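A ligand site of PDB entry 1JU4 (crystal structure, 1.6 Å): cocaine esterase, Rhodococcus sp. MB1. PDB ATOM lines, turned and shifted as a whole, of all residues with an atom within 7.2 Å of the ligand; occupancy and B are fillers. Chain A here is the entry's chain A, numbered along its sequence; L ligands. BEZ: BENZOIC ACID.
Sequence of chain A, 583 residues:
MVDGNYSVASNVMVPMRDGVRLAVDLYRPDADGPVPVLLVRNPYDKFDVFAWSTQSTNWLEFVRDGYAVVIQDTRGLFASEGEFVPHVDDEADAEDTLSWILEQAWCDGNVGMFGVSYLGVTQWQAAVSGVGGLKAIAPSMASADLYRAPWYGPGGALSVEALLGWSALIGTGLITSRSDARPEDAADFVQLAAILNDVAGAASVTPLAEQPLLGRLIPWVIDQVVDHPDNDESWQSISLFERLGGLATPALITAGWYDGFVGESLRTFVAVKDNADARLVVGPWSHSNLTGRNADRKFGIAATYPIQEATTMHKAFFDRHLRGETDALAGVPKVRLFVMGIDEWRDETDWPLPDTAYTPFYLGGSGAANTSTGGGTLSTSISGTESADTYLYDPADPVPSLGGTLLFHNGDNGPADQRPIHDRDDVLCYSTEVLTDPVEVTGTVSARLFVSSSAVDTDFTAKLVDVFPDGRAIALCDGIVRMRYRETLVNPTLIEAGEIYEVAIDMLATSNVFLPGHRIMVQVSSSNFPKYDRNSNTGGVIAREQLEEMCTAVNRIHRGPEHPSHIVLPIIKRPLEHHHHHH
OH of Tyr 44 lies within hydrogen-bond range of O1 of the ligand (2.5 Å).
An oxygen (O1) of the ligand is in hydrogen-bond range of the backbone NH (N) of Tyr 118 (3.0 Å).
The side-chain hydroxyl (OH) of Tyr 44 lies within hydrogen-bond range of the indole nitrogen (NE1) of Trp 166, at 2.8 Å.
The side-chain hydroxyl (OH) of Tyr 118 is in hydrogen-bond range of the backbone NH (N) of His 87 (3.1 Å).
O of Leu 146 lies within hydrogen-bond range of N of Trp 151, at 3.2 Å.
Ser 117 touches the ligand.
CG of Pro 150 touches C4 of the ligand (3.8 Å).
Trp 151 touches the ligand (CH2 to C5, 3.5 Å).
Trp 166 touches the ligand (NE1 to C6, 3.3 Å).
Phe 261 touches the ligand.
His 287 touches the ligand (CE1 to O2, 3.1 Å).
Leu 407 touches the ligand.
CZ of Phe 408 touches C3 of the ligand, 3.8 Å away.
Hydrophobic or aromatic side chains that line the ligand: Tyr 44, Tyr 118, Pro 150, Trp 151, Trp 166, Phe 261, His 287, Leu 407 and Phe 408.
Within 4 Å of the ligand: Tyr 44, Ser 117, Tyr 118, Pro 150, Trp 151, Trp 166, Phe 261, His 287, Leu 407 and Phe 408.
The nearest printed residue that does not touch the ligand is Val 116 (4.5 Å).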
ATOM      1  N   PRO A  43      -2.693 -10.826 -10.348  1.00  0.00           N
ATOM      2  CA  PRO A  43      -1.934 -12.051 -10.530  1.00  0.00           C
ATOM      3  C   PRO A  43      -0.588 -11.811 -11.185  1.00  0.00           C
ATOM      4  O   PRO A  43       0.082 -12.785 -11.565  1.00  0.00           O
ATOM      5  CB  PRO A  43      -2.843 -12.869 -11.485  1.00  0.00           C
ATOM      6  CG  PRO A  43      -3.463 -11.800 -12.335  1.00  0.00           C
ATOM      7  CD  PRO A  43      -3.534 -10.550 -11.526  1.00  0.00           C
ATOM      8  N   TYR A  44      -0.187 -10.560 -11.377  1.00  0.00           N
ATOM      9  CA  TYR A  44       1.080 -10.264 -12.081  1.00  0.00           C
ATOM     10  C   TYR A  44       2.108  -9.617 -11.162  1.00  0.00           C
ATOM     11  O   TYR A  44       2.917  -8.829 -11.663  1.00  0.00           O
ATOM     12  CB  TYR A  44       0.745  -9.366 -13.262  1.00  0.00           C
ATOM     13  CG  TYR A  44      -0.402  -9.824 -14.130  1.00  0.00           C
ATOM     14  CD1 TYR A  44      -0.383 -11.067 -14.753  1.00  0.00           C
ATOM     15  CD2 TYR A  44      -1.537  -9.052 -14.360  1.00  0.00           C
ATOM     16  CE1 TYR A  44      -1.424 -11.517 -15.544  1.00  0.00           C
ATOM     17  CE2 TYR A  44      -2.587  -9.478 -15.152  1.00  0.00           C
ATOM     18  CZ  TYR A  44      -2.524 -10.717 -15.749  1.00  0.00           C
ATOM     19  OH  TYR A  44      -3.553 -11.137 -16.548  1.00  0.00           O
ATOM     20  N   HIS A  87      -9.503 -17.775 -11.891  1.00  0.00           N
ATOM     21  CA  HIS A  87     -10.854 -17.379 -11.596  1.00  0.00           C
ATOM     22  C   HIS A  87     -11.562 -18.109 -10.466  1.00  0.00           C
ATOM     23  O   HIS A  87     -12.397 -17.497  -9.799  1.00  0.00           O
ATOM     24  CB  HIS A  87     -11.813 -17.555 -12.819  1.00  0.00           C
ATOM     25  CG  HIS A  87     -11.223 -16.846 -14.001  1.00  0.00           C
ATOM     26  ND1 HIS A  87     -10.965 -17.502 -15.193  1.00  0.00           N
ATOM     27  CD2 HIS A  87     -10.791 -15.573 -14.144  1.00  0.00           C
ATOM     28  CE1 HIS A  87     -10.423 -16.564 -15.925  1.00  0.00           C
ATOM     29  NE2 HIS A  87     -10.316 -15.382 -15.402  1.00  0.00           N
ATOM     30  N   VAL A 116      -7.416  -3.107 -14.158  1.00  0.00           N
ATOM     31  CA  VAL A 116      -7.625  -3.420 -15.570  1.00  0.00           C
ATOM     32  C   VAL A 116      -7.452  -4.897 -15.873  1.00  0.00           C
ATOM     33  O   VAL A 116      -6.604  -5.595 -15.305  1.00  0.00           O
ATOM     34  CB  VAL A 116      -6.680  -2.496 -16.407  1.00  0.00           C
ATOM     35  CG1 VAL A 116      -5.229  -2.811 -16.110  1.00  0.00           C
ATOM     36  CG2 VAL A 116      -6.997  -2.601 -17.892  1.00  0.00           C
ATOM     37  N   SER A 117      -8.304  -5.371 -16.761  1.00  0.00           N
ATOM     38  CA  SER A 117      -8.411  -6.741 -17.290  1.00  0.00           C
ATOM     39  C   SER A 117      -8.565  -7.761 -16.172  1.00  0.00           C
ATOM     40  O   SER A 117      -9.635  -7.767 -15.539  1.00  0.00           O
ATOM     41  CB  SER A 117      -7.214  -7.010 -18.207  1.00  0.00           C
ATOM     42  OG  SER A 117      -7.117  -6.006 -19.199  1.00  0.00           O
ATOM     43  N   TYR A 118      -7.614  -8.652 -15.887  1.00  0.00           N
ATOM     44  CA  TYR A 118      -7.871  -9.596 -14.768  1.00  0.00           C
ATOM     45  C   TYR A 118      -8.096  -8.823 -13.469  1.00  0.00           C
ATOM     46  O   TYR A 118      -8.883  -9.241 -12.615  1.00  0.00           O
ATOM     47  CB  TYR A 118      -6.714 -10.564 -14.614  1.00  0.00           C
ATOM     48  CG  TYR A 118      -6.915 -11.816 -13.799  1.00  0.00           C
ATOM     49  CD1 TYR A 118      -6.975 -11.841 -12.420  1.00  0.00           C
ATOM     50  CD2 TYR A 118      -7.026 -13.024 -14.464  1.00  0.00           C
ATOM     51  CE1 TYR A 118      -7.152 -13.047 -11.753  1.00  0.00           C
ATOM     52  CE2 TYR A 118      -7.196 -14.223 -13.798  1.00  0.00           C
ATOM     53  CZ  TYR A 118      -7.262 -14.241 -12.414  1.00  0.00           C
ATOM     54  OH  TYR A 118      -7.439 -15.447 -11.747  1.00  0.00           O
ATOM     55  N   LEU A 119      -7.454  -7.664 -13.354  1.00  0.00           N
ATOM     56  CA  LEU A 119      -7.638  -6.789 -12.196  1.00  0.00           C
ATOM     57  C   LEU A 119      -8.987  -6.063 -12.233  1.00  0.00           C
ATOM     58  O   LEU A 119      -9.379  -5.414 -11.242  1.00  0.00           O
ATOM     59  CB  LEU A 119      -6.529  -5.753 -12.121  1.00  0.00           C
ATOM     60  CG  LEU A 119      -5.117  -6.152 -11.727  1.00  0.00           C
ATOM     61  CD1 LEU A 119      -4.553  -7.197 -12.680  1.00  0.00           C
ATOM     62  CD2 LEU A 119      -4.232  -4.915 -11.707  1.00  0.00           C
ATOM     63  N   GLY A 120      -9.683  -6.140 -13.361  1.00  0.00           N
ATOM     64  CA  GLY A 120     -11.060  -5.698 -13.451  1.00  0.00           C
ATOM     65  C   GLY A 120     -12.029  -6.847 -13.247  1.00  0.00           C
ATOM     66  O   GLY A 120     -13.071  -6.677 -12.601  1.00  0.00           O
ATOM     67  N   VAL A 121     -11.725  -8.033 -13.795  1.00  0.00           N
ATOM     68  CA  VAL A 121     -12.654  -9.149 -13.590  1.00  0.00           C
ATOM     69  C   VAL A 121     -12.840  -9.409 -12.089  1.00  0.00           C
ATOM     70  O   VAL A 121     -13.931  -9.695 -11.591  1.00  0.00           O
ATOM     71  CB  VAL A 121     -12.130 -10.416 -14.288  1.00  0.00           C
ATOM     72  CG1 VAL A 121     -12.881 -11.660 -13.825  1.00  0.00           C
ATOM     73  CG2 VAL A 121     -12.201 -10.260 -15.808  1.00  0.00           C
ATOM     74  N   MET A 141     -11.489  -2.570 -18.940  1.00  0.00           N
ATOM     75  CA  MET A 141     -11.243  -3.651 -19.889  1.00  0.00           C
ATOM     76  C   MET A 141     -11.592  -5.000 -19.292  1.00  0.00           C
ATOM     77  O   MET A 141     -10.802  -5.947 -19.300  1.00  0.00           O
ATOM     78  CB  MET A 141      -9.760  -3.702 -20.312  1.00  0.00           C
ATOM     79  CG  MET A 141      -9.209  -2.328 -20.564  1.00  0.00           C
ATOM     80  SD  MET A 141     -10.119  -1.539 -21.888  1.00  0.00           S
ATOM     81  CE  MET A 141      -9.518   0.149 -21.713  1.00  0.00           C
ATOM     82  N   LEU A 146     -16.792 -14.961 -18.353  1.00  0.00           N
ATOM     83  CA  LEU A 146     -15.475 -15.380 -18.854  1.00  0.00           C
ATOM     84  C   LEU A 146     -15.589 -16.244 -20.097  1.00  0.00           C
ATOM     85  O   LEU A 146     -14.634 -16.244 -20.905  1.00  0.00           O
ATOM     86  CB  LEU A 146     -14.677 -16.072 -17.747  1.00  0.00           C
ATOM     87  CG  LEU A 146     -14.124 -15.176 -16.636  1.00  0.00           C
ATOM     88  CD1 LEU A 146     -13.466 -13.892 -17.145  1.00  0.00           C
ATOM     89  CD2 LEU A 146     -15.229 -14.862 -15.670  1.00  0.00           C
ATOM     90  N   PRO A 150     -12.707 -13.382 -21.896  1.00  0.00           N
ATOM     91  CA  PRO A 150     -11.973 -13.470 -23.159  1.00  0.00           C
ATOM     92  C   PRO A 150     -11.824 -14.844 -23.776  1.00  0.00           C
ATOM     93  O   PRO A 150     -11.151 -14.978 -24.807  1.00  0.00           O
ATOM     94  CB  PRO A 150     -10.578 -12.991 -22.711  1.00  0.00           C
ATOM     95  CG  PRO A 150     -10.442 -13.606 -21.347  1.00  0.00           C
ATOM     96  CD  PRO A 150     -11.822 -13.696 -20.761  1.00  0.00           C
ATOM     97  N   TRP A 151     -12.411 -15.904 -23.228  1.00  0.00           N
ATOM     98  CA  TRP A 151     -11.956 -17.225 -23.691  1.00  0.00           C
ATOM     99  C   TRP A 151     -12.730 -17.817 -24.831  1.00  0.00           C
ATOM    100  O   TRP A 151     -12.071 -18.459 -25.673  1.00  0.00           O
ATOM    101  CB  TRP A 151     -11.951 -18.258 -22.550  1.00  0.00           C
ATOM    102  CG  TRP A 151     -11.146 -17.716 -21.428  1.00  0.00           C
ATOM    103  CD1 TRP A 151     -11.702 -17.667 -20.169  1.00  0.00           C
ATOM    104  CD2 TRP A 151      -9.815 -17.188 -21.392  1.00  0.00           C
ATOM    105  NE1 TRP A 151     -10.739 -17.123 -19.440  1.00  0.00           N
ATOM    106  CE2 TRP A 151      -9.561 -16.804 -20.051  1.00  0.00           C
ATOM    107  CE3 TRP A 151      -8.789 -16.966 -22.311  1.00  0.00           C
ATOM    108  CZ2 TRP A 151      -8.352 -16.243 -19.629  1.00  0.00           C
ATOM    109  CZ3 TRP A 151      -7.581 -16.419 -21.892  1.00  0.00           C
ATOM    110  CH2 TRP A 151      -7.352 -16.040 -20.551  1.00  0.00           C
ATOM    111  N   ALA A 162      -6.002 -15.783 -27.637  1.00  0.00           N
ATOM    112  CA  ALA A 162      -6.133 -15.225 -26.293  1.00  0.00           C
ATOM    113  C   ALA A 162      -5.673 -16.235 -25.248  1.00  0.00           C
ATOM    114  O   ALA A 162      -4.943 -15.943 -24.307  1.00  0.00           O
ATOM    115  CB  ALA A 162      -7.585 -14.820 -26.027  1.00  0.00           C
ATOM    116  N   LEU A 163      -6.145 -17.458 -25.403  1.00  0.00           N
ATOM    117  CA  LEU A 163      -5.867 -18.519 -24.445  1.00  0.00           C
ATOM    118  C   LEU A 163      -4.387 -18.873 -24.402  1.00  0.00           C
ATOM    119  O   LEU A 163      -3.765 -18.935 -23.335  1.00  0.00           O
ATOM    120  CB  LEU A 163      -6.698 -19.751 -24.797  1.00  0.00           C
ATOM    121  CG  LEU A 163      -6.445 -20.967 -23.881  1.00  0.00           C
ATOM    122  CD1 LEU A 163      -6.787 -20.607 -22.444  1.00  0.00           C
ATOM    123  CD2 LEU A 163      -7.239 -22.121 -24.434  1.00  0.00           C
ATOM    124  N   TRP A 166      -2.155 -15.778 -23.284  1.00  0.00           N
ATOM    125  CA  TRP A 166      -2.219 -15.501 -21.855  1.00  0.00           C
ATOM    126  C   TRP A 166      -1.578 -16.628 -21.042  1.00  0.00           C
ATOM    127  O   TRP A 166      -0.877 -16.342 -20.065  1.00  0.00           O
ATOM    128  CB  TRP A 166      -3.640 -15.285 -21.382  1.00  0.00           C
ATOM    129  CG  TRP A 166      -3.770 -14.771 -19.970  1.00  0.00           C
ATOM    130  CD1 TRP A 166      -3.533 -13.517 -19.501  1.00  0.00           C
ATOM    131  CD2 TRP A 166      -4.189 -15.531 -18.826  1.00  0.00           C
ATOM    132  NE1 TRP A 166      -3.766 -13.442 -18.138  1.00  0.00           N
ATOM    133  CE2 TRP A 166      -4.173 -14.666 -17.708  1.00  0.00           C
ATOM    134  CE3 TRP A 166      -4.576 -16.874 -18.655  1.00  0.00           C
ATOM    135  CZ2 TRP A 166      -4.518 -15.082 -16.414  1.00  0.00           C
ATOM    136  CZ3 TRP A 166      -4.917 -17.284 -17.385  1.00  0.00           C
ATOM    137  CH2 TRP A 166      -4.879 -16.391 -16.303  1.00  0.00           C
ATOM    138  N   LEU A 169       2.082 -16.329 -21.003  1.00  0.00           N
ATOM    139  CA  LEU A 169       2.550 -15.220 -20.181  1.00  0.00           C
ATOM    140  C   LEU A 169       2.462 -15.557 -18.703  1.00  0.00           C
ATOM    141  O   LEU A 169       3.368 -15.246 -17.920  1.00  0.00           O
ATOM    142  CB  LEU A 169       1.704 -13.986 -20.514  1.00  0.00           C
ATOM    143  CG  LEU A 169       2.090 -13.250 -21.796  1.00  0.00           C
ATOM    144  CD1 LEU A 169       0.999 -12.273 -22.208  1.00  0.00           C
ATOM    145  CD2 LEU A 169       3.415 -12.505 -21.653  1.00  0.00           C
ATOM    146  N   PHE A 261     -11.974  -7.435 -24.453  1.00  0.00           N
ATOM    147  CA  PHE A 261     -13.109  -7.501 -23.531  1.00  0.00           C
ATOM    148  C   PHE A 261     -14.290  -6.602 -23.853  1.00  0.00           C
ATOM    149  O   PHE A 261     -15.271  -6.626 -23.084  1.00  0.00           O
ATOM    150  CB  PHE A 261     -12.565  -7.146 -22.153  1.00  0.00           C
ATOM    151  CG  PHE A 261     -11.532  -8.103 -21.583  1.00  0.00           C
ATOM    152  CD1 PHE A 261     -10.207  -7.947 -21.920  1.00  0.00           C
ATOM    153  CD2 PHE A 261     -11.902  -9.120 -20.738  1.00  0.00           C
ATOM    154  CE1 PHE A 261      -9.237  -8.782 -21.412  1.00  0.00           C
ATOM    155  CE2 PHE A 261     -10.929  -9.970 -20.225  1.00  0.00           C
ATOM    156  CZ  PHE A 261      -9.603  -9.801 -20.559  1.00  0.00           C
ATOM    157  N   HIS A 287      -5.734  -4.064 -26.467  1.00  0.00           N
ATOM    158  CA  HIS A 287      -5.254  -4.429 -25.130  1.00  0.00           C
ATOM    159  C   HIS A 287      -3.814  -4.017 -24.916  1.00  0.00           C
ATOM    160  O   HIS A 287      -3.456  -3.494 -23.848  1.00  0.00           O
ATOM    161  CB  HIS A 287      -5.476  -5.929 -24.978  1.00  0.00           C
ATOM    162  CG  HIS A 287      -4.643  -6.585 -23.946  1.00  0.00           C
ATOM    163  ND1 HIS A 287      -4.904  -6.512 -22.592  1.00  0.00           N
ATOM    164  CD2 HIS A 287      -3.536  -7.350 -24.089  1.00  0.00           C
ATOM    165  CE1 HIS A 287      -3.978  -7.218 -21.960  1.00  0.00           C
ATOM    166  NE2 HIS A 287      -3.133  -7.726 -22.832  1.00  0.00           N
ATOM    167  N   LEU A 407      -5.763 -10.131 -28.979  1.00  0.00           N
ATOM    168  CA  LEU A 407      -5.104  -9.774 -27.723  1.00  0.00           C
ATOM    169  C   LEU A 407      -3.594  -9.927 -27.742  1.00  0.00           C
ATOM    170  O   LEU A 407      -2.899  -9.000 -27.306  1.00  0.00           O
ATOM    171  CB  LEU A 407      -5.694 -10.638 -26.595  1.00  0.00           C
ATOM    172  CG  LEU A 407      -7.069 -10.220 -26.100  1.00  0.00           C
ATOM    173  CD1 LEU A 407      -7.691 -11.310 -25.246  1.00  0.00           C
ATOM    174  CD2 LEU A 407      -6.977  -8.927 -25.323  1.00  0.00           C
ATOM    175  N   PHE A 408      -3.089 -11.081 -28.195  1.00  0.00           N
ATOM    176  CA  PHE A 408      -1.657 -11.394 -28.118  1.00  0.00           C
ATOM    177  C   PHE A 408      -1.020 -11.618 -29.475  1.00  0.00           C
ATOM    178  O   PHE A 408       0.162 -11.287 -29.662  1.00  0.00           O
ATOM    179  CB  PHE A 408      -1.433 -12.645 -27.232  1.00  0.00           C
ATOM    180  CG  PHE A 408      -1.897 -12.340 -25.821  1.00  0.00           C
ATOM    181  CD1 PHE A 408      -1.218 -11.424 -25.039  1.00  0.00           C
ATOM    182  CD2 PHE A 408      -3.033 -12.959 -25.347  1.00  0.00           C
ATOM    183  CE1 PHE A 408      -1.668 -11.133 -23.764  1.00  0.00           C
ATOM    184  CE2 PHE A 408      -3.467 -12.684 -24.073  1.00  0.00           C
ATOM    185  CZ  PHE A 408      -2.783 -11.801 -23.279  1.00  0.00           C
HETATM  186  C   BEZ L   1      -4.998  -9.414 -18.550  1.00  0.00           C
HETATM  187  O1  BEZ L   1      -5.126  -9.320 -17.345  1.00  0.00           O
HETATM  188  O2  BEZ L   1      -4.558  -8.452 -19.181  1.00  0.00           O
HETATM  189  C1  BEZ L   1      -5.752 -10.421 -19.378  1.00  0.00           C
HETATM  190  C2  BEZ L   1      -5.528 -10.285 -20.737  1.00  0.00           C
HETATM  191  C3  BEZ L   1      -6.171 -11.346 -21.565  1.00  0.00           C
HETATM  192  C4  BEZ L   1      -6.792 -12.497 -20.990  1.00  0.00           C
HETATM  193  C5  BEZ L   1      -6.966 -12.646 -19.591  1.00  0.00           C
HETATM  194  C6  BEZ L   1      -6.448 -11.569 -18.813  1.00  0.00           C
